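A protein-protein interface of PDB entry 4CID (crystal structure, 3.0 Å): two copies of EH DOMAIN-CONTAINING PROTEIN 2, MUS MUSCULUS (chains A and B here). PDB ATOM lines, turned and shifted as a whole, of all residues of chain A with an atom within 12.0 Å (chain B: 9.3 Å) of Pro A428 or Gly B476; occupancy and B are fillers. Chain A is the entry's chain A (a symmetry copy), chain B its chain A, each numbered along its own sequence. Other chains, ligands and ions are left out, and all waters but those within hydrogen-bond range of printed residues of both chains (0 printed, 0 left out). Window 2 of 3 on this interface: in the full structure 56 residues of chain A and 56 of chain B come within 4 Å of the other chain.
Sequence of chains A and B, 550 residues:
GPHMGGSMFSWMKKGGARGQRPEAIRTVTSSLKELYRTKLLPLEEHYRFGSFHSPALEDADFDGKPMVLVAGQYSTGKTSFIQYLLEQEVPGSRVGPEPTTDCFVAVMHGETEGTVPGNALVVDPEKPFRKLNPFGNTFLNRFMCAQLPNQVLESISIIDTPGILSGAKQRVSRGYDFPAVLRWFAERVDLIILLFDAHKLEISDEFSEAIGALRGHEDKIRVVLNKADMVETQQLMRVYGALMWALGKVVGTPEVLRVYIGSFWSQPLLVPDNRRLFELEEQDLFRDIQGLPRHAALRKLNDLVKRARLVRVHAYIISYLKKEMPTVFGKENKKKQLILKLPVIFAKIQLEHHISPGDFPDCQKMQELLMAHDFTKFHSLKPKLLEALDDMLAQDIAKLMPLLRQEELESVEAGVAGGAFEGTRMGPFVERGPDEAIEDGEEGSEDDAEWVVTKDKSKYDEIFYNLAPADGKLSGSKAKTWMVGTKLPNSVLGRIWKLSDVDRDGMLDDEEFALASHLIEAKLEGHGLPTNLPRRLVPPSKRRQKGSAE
No position is printed for both chains.
The backbone carbonyl oxygen (O) of Pro A428 lies within hydrogen-bond range of the side-chain amino group (NZ) of Lys B480, at 3.4 Å.
Of the 12 printed residues of chain A, 6 touch a printed residue of chain B. Of the 25 printed residues of chain B, 9 touch a printed residue of chain A. Among the printed residues, 12 pairs touch across the chains. Among the printed residues, no Asp or Glu carboxylate lies within 4 Å of a Lys or Arg side-chain nitrogen of the other chain.
Lys B498 touches Arg A275. Thr A424 touches Gly B506 (O to CA, 3.7 Å). Arg A425 touches Asp B505 (CA to O, 3.8 Å). N of Gly B506 touches O of Arg A425 (3.6 Å). O of Gly B476 touches CG of Pro A428, at 3.6 Å. Trp B497 touches Pro A428 (CE2 to CD, 3.5 Å). CE2 of Phe A429 touches ND2 of Asn B490, 3.5 Å away. Phe A429 touches Leu B493. Gly B494 touches Phe A429 (N to CD2, 3.8 Å). Phe A429 touches Trp B497.
The side-chain amino group of Lys B473 is in salt-bridge range of the side-chain carboxylate of Asp B505, at 3.6 Å. N of Gly B476 sits at hydrogen-bond distance from O of Gly B506. The side-chain carboxylate (OE2) of Glu A87 lies within salt-bridge range of the guanidinium group (NE) of Arg A425, 3.6 Å away. OD2 of Asp B501 is in hydrogen-bond range of N of Gly B506 (2.9 Å).
Of the printed residues of chain B, Arg A425 touches Asp B505 (3.8 Å) and Gly B506 (3.6 Å). Gly A427 touches just one residue of chain B: Trp B497 (3.5 Å). Of chain B, only Gly B476, Lys B480 and Trp B497 come within 4 Å of Pro A428. Ser B475 touches none of the printed residues of chain A. Of chain A, only Pro A428 (3.6 Å) comes within 4 Å of Gly B476. No residue of chain A comes within 4 Å of Ala B479. Of the printed residues of chain A, Lys B480 touches Pro A428 (3.4 Å). No residue of chain A comes within 4 Å of Met B507. Leu B508 touches none of the printed residues of chain A. The nearest residue of chain B that does not touch Pro A428 is Ser B477 (4.5 Å). The nearest printed residue of chain A that does not touch Gly B476 is Gly A427 (6.1 Å).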
ATOM      1  N   GLU A  87      13.647 -22.049  -4.660  1.00  0.00           N
ATOM      2  CA  GLU A  87      14.651 -22.848  -3.950  1.00  0.00           C
ATOM      3  C   GLU A  87      14.293 -24.335  -4.034  1.00  0.00           C
ATOM      4  O   GLU A  87      14.431 -25.071  -3.062  1.00  0.00           O
ATOM      5  CB  GLU A  87      14.839 -22.390  -2.490  1.00  0.00           C
ATOM      6  CG  GLU A  87      15.873 -21.278  -2.311  1.00  0.00           C
ATOM      7  CD  GLU A  87      16.440 -21.185  -0.893  1.00  0.00           C
ATOM      8  OE1 GLU A  87      16.533 -22.221  -0.195  1.00  0.00           O
ATOM      9  OE2 GLU A  87      16.815 -20.067  -0.473  1.00  0.00           O
ATOM     10  N   ARG A 275      29.023  -7.505  -6.740  1.00  0.00           N
ATOM     11  CA  ARG A 275      28.169  -8.325  -5.875  1.00  0.00           C
ATOM     12  C   ARG A 275      27.039  -7.534  -5.191  1.00  0.00           C
ATOM     13  O   ARG A 275      25.894  -7.990  -5.146  1.00  0.00           O
ATOM     14  CB  ARG A 275      29.020  -9.030  -4.816  1.00  0.00           C
ATOM     15  CG  ARG A 275      28.208  -9.806  -3.800  1.00  0.00           C
ATOM     16  CD  ARG A 275      29.056 -10.750  -2.971  1.00  0.00           C
ATOM     17  NE  ARG A 275      28.202 -11.607  -2.147  1.00  0.00           N
ATOM     18  CZ  ARG A 275      28.633 -12.596  -1.363  1.00  0.00           C
ATOM     19  NH1 ARG A 275      29.932 -12.883  -1.270  1.00  0.00           N
ATOM     20  NH2 ARG A 275      27.753 -13.306  -0.661  1.00  0.00           N
ATOM     21  N   GLN A 283      16.621  -7.971  -4.470  1.00  0.00           N
ATOM     22  CA  GLN A 283      15.664  -7.539  -3.450  1.00  0.00           C
ATOM     23  C   GLN A 283      14.582  -6.626  -4.020  1.00  0.00           C
ATOM     24  O   GLN A 283      13.405  -6.774  -3.675  1.00  0.00           O
ATOM     25  CB  GLN A 283      16.380  -6.830  -2.296  1.00  0.00           C
ATOM     26  CG  GLN A 283      17.215  -7.755  -1.422  1.00  0.00           C
ATOM     27  CD  GLN A 283      17.924  -7.031  -0.285  1.00  0.00           C
ATOM     28  OE1 GLN A 283      17.886  -7.479   0.863  1.00  0.00           O
ATOM     29  NE2 GLN A 283      18.576  -5.909  -0.597  1.00  0.00           N
ATOM     30  N   GLU A 422      12.322 -15.374   1.977  1.00  0.00           N
ATOM     31  CA  GLU A 422      12.579 -15.389   3.409  1.00  0.00           C
ATOM     32  C   GLU A 422      13.754 -14.477   3.780  1.00  0.00           C
ATOM     33  O   GLU A 422      14.755 -14.406   3.062  1.00  0.00           O
ATOM     34  CB  GLU A 422      12.836 -16.819   3.882  1.00  0.00           C
ATOM     35  CG  GLU A 422      12.670 -17.001   5.380  1.00  0.00           C
ATOM     36  CD  GLU A 422      12.695 -18.458   5.810  1.00  0.00           C
ATOM     37  OE1 GLU A 422      12.851 -19.340   4.935  1.00  0.00           O
ATOM     38  OE2 GLU A 422      12.558 -18.722   7.027  1.00  0.00           O
ATOM     39  N   GLY A 423      13.607 -13.773   4.900  1.00  0.00           N
ATOM     40  CA  GLY A 423      14.587 -12.782   5.339  1.00  0.00           C
ATOM     41  C   GLY A 423      15.887 -13.382   5.836  1.00  0.00           C
ATOM     42  O   GLY A 423      16.961 -12.827   5.591  1.00  0.00           O
ATOM     43  N   THR A 424      15.787 -14.522   6.519  1.00  0.00           N
ATOM     44  CA  THR A 424      16.952 -15.220   7.079  1.00  0.00           C
ATOM     45  C   THR A 424      18.015 -15.532   6.026  1.00  0.00           C
ATOM     46  O   THR A 424      19.210 -15.623   6.335  1.00  0.00           O
ATOM     47  CB  THR A 424      16.538 -16.545   7.736  1.00  0.00           C
ATOM     48  OG1 THR A 424      15.781 -17.319   6.802  1.00  0.00           O
ATOM     49  CG2 THR A 424      15.703 -16.298   8.979  1.00  0.00           C
ATOM     50  N   ARG A 425      17.571 -15.691   4.784  1.00  0.00           N
ATOM     51  CA  ARG A 425      18.457 -15.921   3.643  1.00  0.00           C
ATOM     52  C   ARG A 425      19.617 -14.922   3.539  1.00  0.00           C
ATOM     53  O   ARG A 425      20.689 -15.287   3.080  1.00  0.00           O
ATOM     54  CB  ARG A 425      17.635 -15.911   2.350  1.00  0.00           C
ATOM     55  CG  ARG A 425      18.379 -16.407   1.127  1.00  0.00           C
ATOM     56  CD  ARG A 425      17.426 -16.655  -0.029  1.00  0.00           C
ATOM     57  NE  ARG A 425      18.142 -16.810  -1.294  1.00  0.00           N
ATOM     58  CZ  ARG A 425      18.654 -15.808  -2.011  1.00  0.00           C
ATOM     59  NH1 ARG A 425      18.543 -14.545  -1.608  1.00  0.00           N
ATOM     60  NH2 ARG A 425      19.290 -16.072  -3.143  1.00  0.00           N
ATOM     61  N   MET A 426      19.414 -13.677   3.968  1.00  0.00           N
ATOM     62  CA  MET A 426      20.494 -12.674   3.949  1.00  0.00           C
ATOM     63  C   MET A 426      21.564 -12.918   4.991  1.00  0.00           C
ATOM     64  O   MET A 426      22.627 -12.303   4.929  1.00  0.00           O
ATOM     65  CB  MET A 426      19.968 -11.246   4.155  1.00  0.00           C
ATOM     66  CG  MET A 426      19.292 -10.656   2.914  1.00  0.00           C
ATOM     67  SD  MET A 426      20.567 -10.298   1.436  1.00  0.00           S
ATOM     68  CE  MET A 426      21.679  -8.846   2.165  1.00  0.00           C
ATOM     69  N   GLY A 427      21.300 -13.794   5.959  1.00  0.00           N
ATOM     70  CA  GLY A 427      22.284 -14.143   6.985  1.00  0.00           C
ATOM     71  C   GLY A 427      21.941 -13.532   8.334  1.00  0.00           C
ATOM     72  O   GLY A 427      21.153 -12.591   8.405  1.00  0.00           O
ATOM     73  N   PRO A 428      22.539 -14.053   9.421  1.00  0.00           N
ATOM     74  CA  PRO A 428      22.195 -13.601  10.762  1.00  0.00           C
ATOM     75  C   PRO A 428      22.993 -12.392  11.269  1.00  0.00           C
ATOM     76  O   PRO A 428      22.835 -12.019  12.430  1.00  0.00           O
ATOM     77  CB  PRO A 428      22.509 -14.829  11.612  1.00  0.00           C
ATOM     78  CG  PRO A 428      23.672 -15.450  10.927  1.00  0.00           C
ATOM     79  CD  PRO A 428      23.559 -15.116   9.461  1.00  0.00           C
ATOM     80  N   PHE A 429      23.840 -11.793  10.431  1.00  0.00           N
ATOM     81  CA  PHE A 429      24.609 -10.606  10.825  1.00  0.00           C
ATOM     82  C   PHE A 429      24.044  -9.366  10.146  1.00  0.00           C
ATOM     83  O   PHE A 429      23.923  -9.327   8.923  1.00  0.00           O
ATOM     84  CB  PHE A 429      26.084 -10.771  10.464  1.00  0.00           C
ATOM     85  CG  PHE A 429      26.770 -11.873  11.222  1.00  0.00           C
ATOM     86  CD1 PHE A 429      26.639 -13.194  10.821  1.00  0.00           C
ATOM     87  CD2 PHE A 429      27.546 -11.591  12.336  1.00  0.00           C
ATOM     88  CE1 PHE A 429      27.269 -14.211  11.518  1.00  0.00           C
ATOM     89  CE2 PHE A 429      28.177 -12.603  13.035  1.00  0.00           C
ATOM     90  CZ  PHE A 429      28.039 -13.915  12.625  1.00  0.00           C
ATOM     91  N   VAL A 430      23.698  -8.365  10.955  1.00  0.00           N
ATOM     92  CA  VAL A 430      23.065  -7.119  10.491  1.00  0.00           C
ATOM     93  C   VAL A 430      21.686  -7.381   9.874  1.00  0.00           C
ATOM     94  O   VAL A 430      21.569  -7.939   8.783  1.00  0.00           O
ATOM     95  CB  VAL A 430      23.964  -6.331   9.504  1.00  0.00           C
ATOM     96  CG1 VAL A 430      23.362  -4.962   9.198  1.00  0.00           C
ATOM     97  CG2 VAL A 430      25.370  -6.172  10.070  1.00  0.00           C
ATOM     98  N   PRO B 469      22.675 -29.801  13.245  1.00  0.00           N
ATOM     99  CA  PRO B 469      22.117 -29.197  12.047  1.00  0.00           C
ATOM    100  C   PRO B 469      21.005 -30.089  11.542  1.00  0.00           C
ATOM    101  O   PRO B 469      21.094 -31.304  11.687  1.00  0.00           O
ATOM    102  CB  PRO B 469      23.293 -29.196  11.072  1.00  0.00           C
ATOM    103  CG  PRO B 469      24.129 -30.353  11.495  1.00  0.00           C
ATOM    104  CD  PRO B 469      23.951 -30.490  12.978  1.00  0.00           C
ATOM    105  N   LYS B 473      22.155 -29.256   7.363  1.00  0.00           N
ATOM    106  CA  LYS B 473      22.233 -27.809   7.239  1.00  0.00           C
ATOM    107  C   LYS B 473      22.067 -27.152   8.595  1.00  0.00           C
ATOM    108  O   LYS B 473      21.078 -27.382   9.296  1.00  0.00           O
ATOM    109  CB  LYS B 473      21.166 -27.302   6.276  1.00  0.00           C
ATOM    110  CG  LYS B 473      21.490 -27.595   4.823  1.00  0.00           C
ATOM    111  CD  LYS B 473      20.392 -27.117   3.886  1.00  0.00           C
ATOM    112  CE  LYS B 473      20.745 -27.390   2.430  1.00  0.00           C
ATOM    113  NZ  LYS B 473      21.790 -26.459   1.909  1.00  0.00           N
ATOM    114  N   LEU B 474      23.064 -26.355   8.962  1.00  0.00           N
ATOM    115  CA  LEU B 474      23.037 -25.596  10.193  1.00  0.00           C
ATOM    116  C   LEU B 474      22.396 -24.245   9.936  1.00  0.00           C
ATOM    117  O   LEU B 474      22.733 -23.554   8.964  1.00  0.00           O
ATOM    118  CB  LEU B 474      24.452 -25.400  10.739  1.00  0.00           C
ATOM    119  CG  LEU B 474      24.564 -24.671  12.081  1.00  0.00           C
ATOM    120  CD1 LEU B 474      23.836 -25.446  13.171  1.00  0.00           C
ATOM    121  CD2 LEU B 474      26.023 -24.458  12.454  1.00  0.00           C
ATOM    122  N   SER B 475      21.474 -23.881  10.822  1.00  0.00           N
ATOM    123  CA  SER B 475      20.789 -22.599  10.772  1.00  0.00           C
ATOM    124  C   SER B 475      21.746 -21.443  11.040  1.00  0.00           C
ATOM    125  O   SER B 475      22.770 -21.607  11.712  1.00  0.00           O
ATOM    126  CB  SER B 475      19.663 -22.574  11.812  1.00  0.00           C
ATOM    127  OG  SER B 475      19.241 -21.250  12.083  1.00  0.00           O
ATOM    128  N   GLY B 476      21.399 -20.273  10.514  1.00  0.00           N
ATOM    129  CA  GLY B 476      22.137 -19.051  10.807  1.00  0.00           C
ATOM    130  C   GLY B 476      22.132 -18.748  12.294  1.00  0.00           C
ATOM    131  O   GLY B 476      23.175 -18.463  12.873  1.00  0.00           O
ATOM    132  N   SER B 477      20.954 -18.828  12.911  1.00  0.00           N
ATOM    133  CA  SER B 477      20.799 -18.615  14.355  1.00  0.00           C
ATOM    134  C   SER B 477      21.791 -19.461  15.143  1.00  0.00           C
ATOM    135  O   SER B 477      22.501 -18.967  16.017  1.00  0.00           O
ATOM    136  CB  SER B 477      19.377 -18.983  14.800  1.00  0.00           C
ATOM    137  OG  SER B 477      18.424 -18.693  13.790  1.00  0.00           O
ATOM    138  N   LYS B 478      21.834 -20.741  14.804  1.00  0.00           N
ATOM    139  CA  LYS B 478      22.672 -21.703  15.502  1.00  0.00           C
ATOM    140  C   LYS B 478      24.148 -21.466  15.160  1.00  0.00           C
ATOM    141  O   LYS B 478      25.027 -21.633  16.011  1.00  0.00           O
ATOM    142  CB  LYS B 478      22.251 -23.131  15.132  1.00  0.00           C
ATOM    143  CG  LYS B 478      20.774 -23.452  15.374  1.00  0.00           C
ATOM    144  CD  LYS B 478      20.490 -23.872  16.811  1.00  0.00           C
ATOM    145  CE  LYS B 478      20.430 -25.385  16.965  1.00  0.00           C
ATOM    146  NZ  LYS B 478      21.688 -26.065  16.548  1.00  0.00           N
ATOM    147  N   ALA B 479      24.412 -21.069  13.917  1.00  0.00           N
ATOM    148  CA  ALA B 479      25.783 -20.818  13.457  1.00  0.00           C
ATOM    149  C   ALA B 479      26.402 -19.600  14.129  1.00  0.00           C
ATOM    150  O   ALA B 479      27.560 -19.634  14.533  1.00  0.00           O
ATOM    151  CB  ALA B 479      25.813 -20.646  11.947  1.00  0.00           C
ATOM    152  N   LYS B 480      25.621 -18.528  14.230  1.00  0.00           N
ATOM    153  CA  LYS B 480      26.054 -17.292  14.880  1.00  0.00           C
ATOM    154  C   LYS B 480      26.371 -17.544  16.345  1.00  0.00           C
ATOM    155  O   LYS B 480      27.448 -17.184  16.832  1.00  0.00           O
ATOM    156  CB  LYS B 480      24.959 -16.228  14.772  1.00  0.00           C
ATOM    157  CG  LYS B 480      25.307 -14.891  15.407  1.00  0.00           C
ATOM    158  CD  LYS B 480      24.207 -13.863  15.194  1.00  0.00           C
ATOM    159  CE  LYS B 480      24.516 -12.559  15.913  1.00  0.00           C
ATOM    160  NZ  LYS B 480      23.420 -11.561  15.777  1.00  0.00           N
ATOM    161  N   THR B 481      25.427 -18.179  17.036  1.00  0.00           N
ATOM    162  CA  THR B 481      25.558 -18.423  18.469  1.00  0.00           C
ATOM    163  C   THR B 481      26.807 -19.252  18.789  1.00  0.00           C
ATOM    164  O   THR B 481      27.378 -19.120  19.871  1.00  0.00           O
ATOM    165  CB  THR B 481      24.278 -19.063  19.070  1.00  0.00           C
ATOM    166  OG1 THR B 481      24.321 -18.980  20.496  1.00  0.00           O
ATOM    167  CG2 THR B 481      24.118 -20.517  18.664  1.00  0.00           C
ATOM    168  N   TRP B 482      27.229 -20.092  17.847  1.00  0.00           N
ATOM    169  CA  TRP B 482      28.497 -20.804  17.981  1.00  0.00           C
ATOM    170  C   TRP B 482      29.675 -19.918  17.615  1.00  0.00           C
ATOM    171  O   TRP B 482      30.644 -19.822  18.370  1.00  0.00           O
ATOM    172  CB  TRP B 482      28.523 -22.037  17.089  1.00  0.00           C
ATOM    173  CG  TRP B 482      29.887 -22.662  16.982  1.00  0.00           C
ATOM    174  CD1 TRP B 482      30.546 -23.370  17.946  1.00  0.00           C
ATOM    175  CD2 TRP B 482      30.753 -22.634  15.843  1.00  0.00           C
ATOM    176  NE1 TRP B 482      31.767 -23.787  17.477  1.00  0.00           N
ATOM    177  CE2 TRP B 482      31.918 -23.348  16.188  1.00  0.00           C
ATOM    178  CE3 TRP B 482      30.655 -22.077  14.563  1.00  0.00           C
ATOM    179  CZ2 TRP B 482      32.977 -23.519  15.300  1.00  0.00           C
ATOM    180  CZ3 TRP B 482      31.708 -22.247  13.680  1.00  0.00           C
ATOM    181  CH2 TRP B 482      32.854 -22.963  14.052  1.00  0.00           C
ATOM    182  N   MET B 483      29.582 -19.299  16.437  1.00  0.00           N
ATOM    183  CA  MET B 483      30.643 -18.443  15.889  1.00  0.00           C
ATOM    184  C   MET B 483      31.089 -17.419  16.903  1.00  0.00           C
ATOM    185  O   MET B 483      32.289 -17.287  17.177  1.00  0.00           O
ATOM    186  CB  MET B 483      30.159 -17.758  14.603  1.00  0.00           C
ATOM    187  CG  MET B 483      30.252 -18.681  13.383  1.00  0.00           C
ATOM    188  SD  MET B 483      29.580 -17.816  11.737  1.00  0.00           S
ATOM    189  CE  MET B 483      31.189 -16.727  11.413  1.00  0.00           C
ATOM    190  N   VAL B 484      30.127 -16.716  17.500  1.00  0.00           N
ATOM    191  CA  VAL B 484      30.434 -15.695  18.511  1.00  0.00           C
ATOM    192  C   VAL B 484      31.241 -16.281  19.683  1.00  0.00           C
ATOM    193  O   VAL B 484      32.074 -15.590  20.284  1.00  0.00           O
ATOM    194  CB  VAL B 484      29.151 -14.990  19.018  1.00  0.00           C
ATOM    195  CG1 VAL B 484      28.406 -15.852  20.033  1.00  0.00           C
ATOM    196  CG2 VAL B 484      29.489 -13.632  19.612  1.00  0.00           C
ATOM    197  N   ASN B 490      32.302  -9.013  15.955  1.00  0.00           N
ATOM    198  CA  ASN B 490      31.117  -9.252  15.132  1.00  0.00           C
ATOM    199  C   ASN B 490      31.365  -8.961  13.653  1.00  0.00           C
ATOM    200  O   ASN B 490      31.022  -9.762  12.776  1.00  0.00           O
ATOM    201  CB  ASN B 490      29.963  -8.387  15.645  1.00  0.00           C
ATOM    202  CG  ASN B 490      28.608  -8.898  15.209  1.00  0.00           C
ATOM    203  OD1 ASN B 490      27.842  -8.184  14.556  1.00  0.00           O
ATOM    204  ND2 ASN B 490      28.296 -10.137  15.578  1.00  0.00           N
ATOM    205  N   LEU B 493      33.346 -11.742  12.047  1.00  0.00           N
ATOM    206  CA  LEU B 493      32.442 -12.891  11.944  1.00  0.00           C
ATOM    207  C   LEU B 493      31.450 -12.730  10.783  1.00  0.00           C
ATOM    208  O   LEU B 493      31.174 -13.694  10.063  1.00  0.00           O
ATOM    209  CB  LEU B 493      31.693 -13.117  13.259  1.00  0.00           C
ATOM    210  CG  LEU B 493      32.553 -13.512  14.459  1.00  0.00           C
ATOM    211  CD1 LEU B 493      31.684 -13.644  15.697  1.00  0.00           C
ATOM    212  CD2 LEU B 493      33.316 -14.803  14.199  1.00  0.00           C
ATOM    213  N   GLY B 494      30.929 -11.517  10.595  1.00  0.00           N
ATOM    214  CA  GLY B 494      30.085 -11.224   9.438  1.00  0.00           C
ATOM    215  C   GLY B 494      30.798 -11.455   8.112  1.00  0.00           C
ATOM    216  O   GLY B 494      30.265 -12.128   7.213  1.00  0.00           O
ATOM    217  N   ILE B 496      33.302 -13.263   7.559  1.00  0.00           N
ATOM    218  CA  ILE B 496      33.464 -14.703   7.427  1.00  0.00           C
ATOM    219  C   ILE B 496      32.162 -15.290   6.908  1.00  0.00           C
ATOM    220  O   ILE B 496      32.153 -15.918   5.858  1.00  0.00           O
ATOM    221  CB  ILE B 496      33.889 -15.363   8.750  1.00  0.00           C
ATOM    222  CG1 ILE B 496      35.327 -14.963   9.075  1.00  0.00           C
ATOM    223  CG2 ILE B 496      33.793 -16.876   8.646  1.00  0.00           C
ATOM    224  CD1 ILE B 496      35.774 -15.279  10.483  1.00  0.00           C
ATOM    225  N   TRP B 497      31.058 -15.046   7.612  1.00  0.00           N
ATOM    226  CA  TRP B 497      29.762 -15.572   7.186  1.00  0.00           C
ATOM    227  C   TRP B 497      29.517 -15.335   5.701  1.00  0.00           C
ATOM    228  O   TRP B 497      29.208 -16.280   4.952  1.00  0.00           O
ATOM    229  CB  TRP B 497      28.614 -14.952   7.975  1.00  0.00           C
ATOM    230  CG  TRP B 497      27.315 -15.406   7.441  1.00  0.00           C
ATOM    231  CD1 TRP B 497      26.571 -14.796   6.483  1.00  0.00           C
ATOM    232  CD2 TRP B 497      26.626 -16.608   7.783  1.00  0.00           C
ATOM    233  NE1 TRP B 497      25.444 -15.532   6.219  1.00  0.00           N
ATOM    234  CE2 TRP B 497      25.455 -16.652   7.005  1.00  0.00           C
ATOM    235  CE3 TRP B 497      26.879 -17.649   8.684  1.00  0.00           C
ATOM    236  CZ2 TRP B 497      24.535 -17.693   7.097  1.00  0.00           C
ATOM    237  CZ3 TRP B 497      25.965 -18.684   8.777  1.00  0.00           C
ATOM    238  CH2 TRP B 497      24.806 -18.699   7.988  1.00  0.00           C
ATOM    239  N   LYS B 498      29.647 -14.072   5.289  1.00  0.00           N
ATOM    240  CA  LYS B 498      29.473 -13.686   3.874  1.00  0.00           C
ATOM    241  C   LYS B 498      30.303 -14.569   2.937  1.00  0.00           C
ATOM    242  O   LYS B 498      29.823 -14.976   1.877  1.00  0.00           O
ATOM    243  CB  LYS B 498      29.860 -12.212   3.666  1.00  0.00           C
ATOM    244  CG  LYS B 498      29.637 -11.659   2.258  1.00  0.00           C
ATOM    245  CD  LYS B 498      28.343 -10.862   2.132  1.00  0.00           C
ATOM    246  CE  LYS B 498      27.113 -11.728   2.349  1.00  0.00           C
ATOM    247  NZ  LYS B 498      25.877 -11.083   1.822  1.00  0.00           N
ATOM    248  N   ASP B 501      28.969 -18.624   3.434  1.00  0.00           N
ATOM    249  CA  ASP B 501      27.671 -19.001   2.870  1.00  0.00           C
ATOM    250  C   ASP B 501      27.700 -18.861   1.348  1.00  0.00           C
ATOM    251  O   ASP B 501      27.153 -17.908   0.789  1.00  0.00           O
ATOM    252  CB  ASP B 501      26.532 -18.177   3.474  1.00  0.00           C
ATOM    253  CG  ASP B 501      25.153 -18.718   3.098  1.00  0.00           C
ATOM    254  OD1 ASP B 501      25.062 -19.812   2.491  1.00  0.00           O
ATOM    255  OD2 ASP B 501      24.151 -18.044   3.410  1.00  0.00           O
ATOM    256  N   ASP B 505      22.028 -19.201   1.044  1.00  0.00           N
ATOM    257  CA  ASP B 505      20.685 -19.617   1.449  1.00  0.00           C
ATOM    258  C   ASP B 505      20.406 -19.325   2.928  1.00  0.00           C
ATOM    259  O   ASP B 505      19.325 -19.630   3.427  1.00  0.00           O
ATOM    260  CB  ASP B 505      20.479 -21.113   1.164  1.00  0.00           C
ATOM    261  CG  ASP B 505      21.247 -22.012   2.127  1.00  0.00           C
ATOM    262  OD1 ASP B 505      22.392 -21.667   2.488  1.00  0.00           O
ATOM    263  OD2 ASP B 505      20.707 -23.071   2.514  1.00  0.00           O
ATOM    264  N   GLY B 506      21.381 -18.751   3.628  1.00  0.00           N
ATOM    265  CA  GLY B 506      21.211 -18.388   5.034  1.00  0.00           C
ATOM    266  C   GLY B 506      21.535 -19.500   6.014  1.00  0.00           C
ATOM    267  O   GLY B 506      21.343 -19.346   7.219  1.00  0.00           O
ATOM    268  N   MET B 507      22.040 -20.617   5.501  1.00  0.00           N
ATOM    269  CA  MET B 507      22.411 -21.758   6.328  1.00  0.00           C
ATOM    270  C   MET B 507      23.786 -22.210   5.942  1.00  0.00           C
ATOM    271  O   MET B 507      24.324 -21.777   4.918  1.00  0.00           O
ATOM    272  CB  MET B 507      21.419 -22.870   6.049  1.00  0.00           C
ATOM    273  CG  MET B 507      19.992 -22.460   6.404  1.00  0.00           C
ATOM    274  SD  MET B 507      18.827 -24.046   6.268  1.00  0.00           S
ATOM    275  CE  MET B 507      17.694 -23.428   4.775  1.00  0.00           C
ATOM    276  N   LEU B 508      24.380 -23.087   6.744  1.00  0.00           N
ATOM    277  CA  LEU B 508      25.690 -23.653   6.398  1.00  0.00           C
ATOM    278  C   LEU B 508      25.653 -25.171   6.405  1.00  0.00           C
ATOM    279  O   LEU B 508      25.325 -25.777   7.418  1.00  0.00           O
ATOM    280  CB  LEU B 508      26.766 -23.171   7.370  1.00  0.00           C
ATOM    281  CG  LEU B 508      27.027 -21.667   7.393  1.00  0.00           C
ATOM    282  CD1 LEU B 508      27.909 -21.313   8.574  1.00  0.00           C
ATOM    283  CD2 LEU B 508      27.670 -21.198   6.101  1.00  0.00           C
ATOM    284  N   ASP B 509      25.985 -25.784   5.273  1.00  0.00           N
ATOM    285  CA  ASP B 509      26.195 -27.229   5.228  1.00  0.00           C
ATOM    286  C   ASP B 509      27.623 -27.551   5.678  1.00  0.00           C
ATOM    287  O   ASP B 509      28.427 -26.651   5.923  1.00  0.00           O
ATOM    288  CB  ASP B 509      25.909 -27.789   3.829  1.00  0.00           C
ATOM    289  CG  ASP B 509      26.881 -27.282   2.775  1.00  0.00           C
ATOM    290  OD1 ASP B 509      28.089 -27.124   3.073  1.00  0.00           O
ATOM    291  OD2 ASP B 509      26.426 -27.051   1.633  1.00  0.00           O
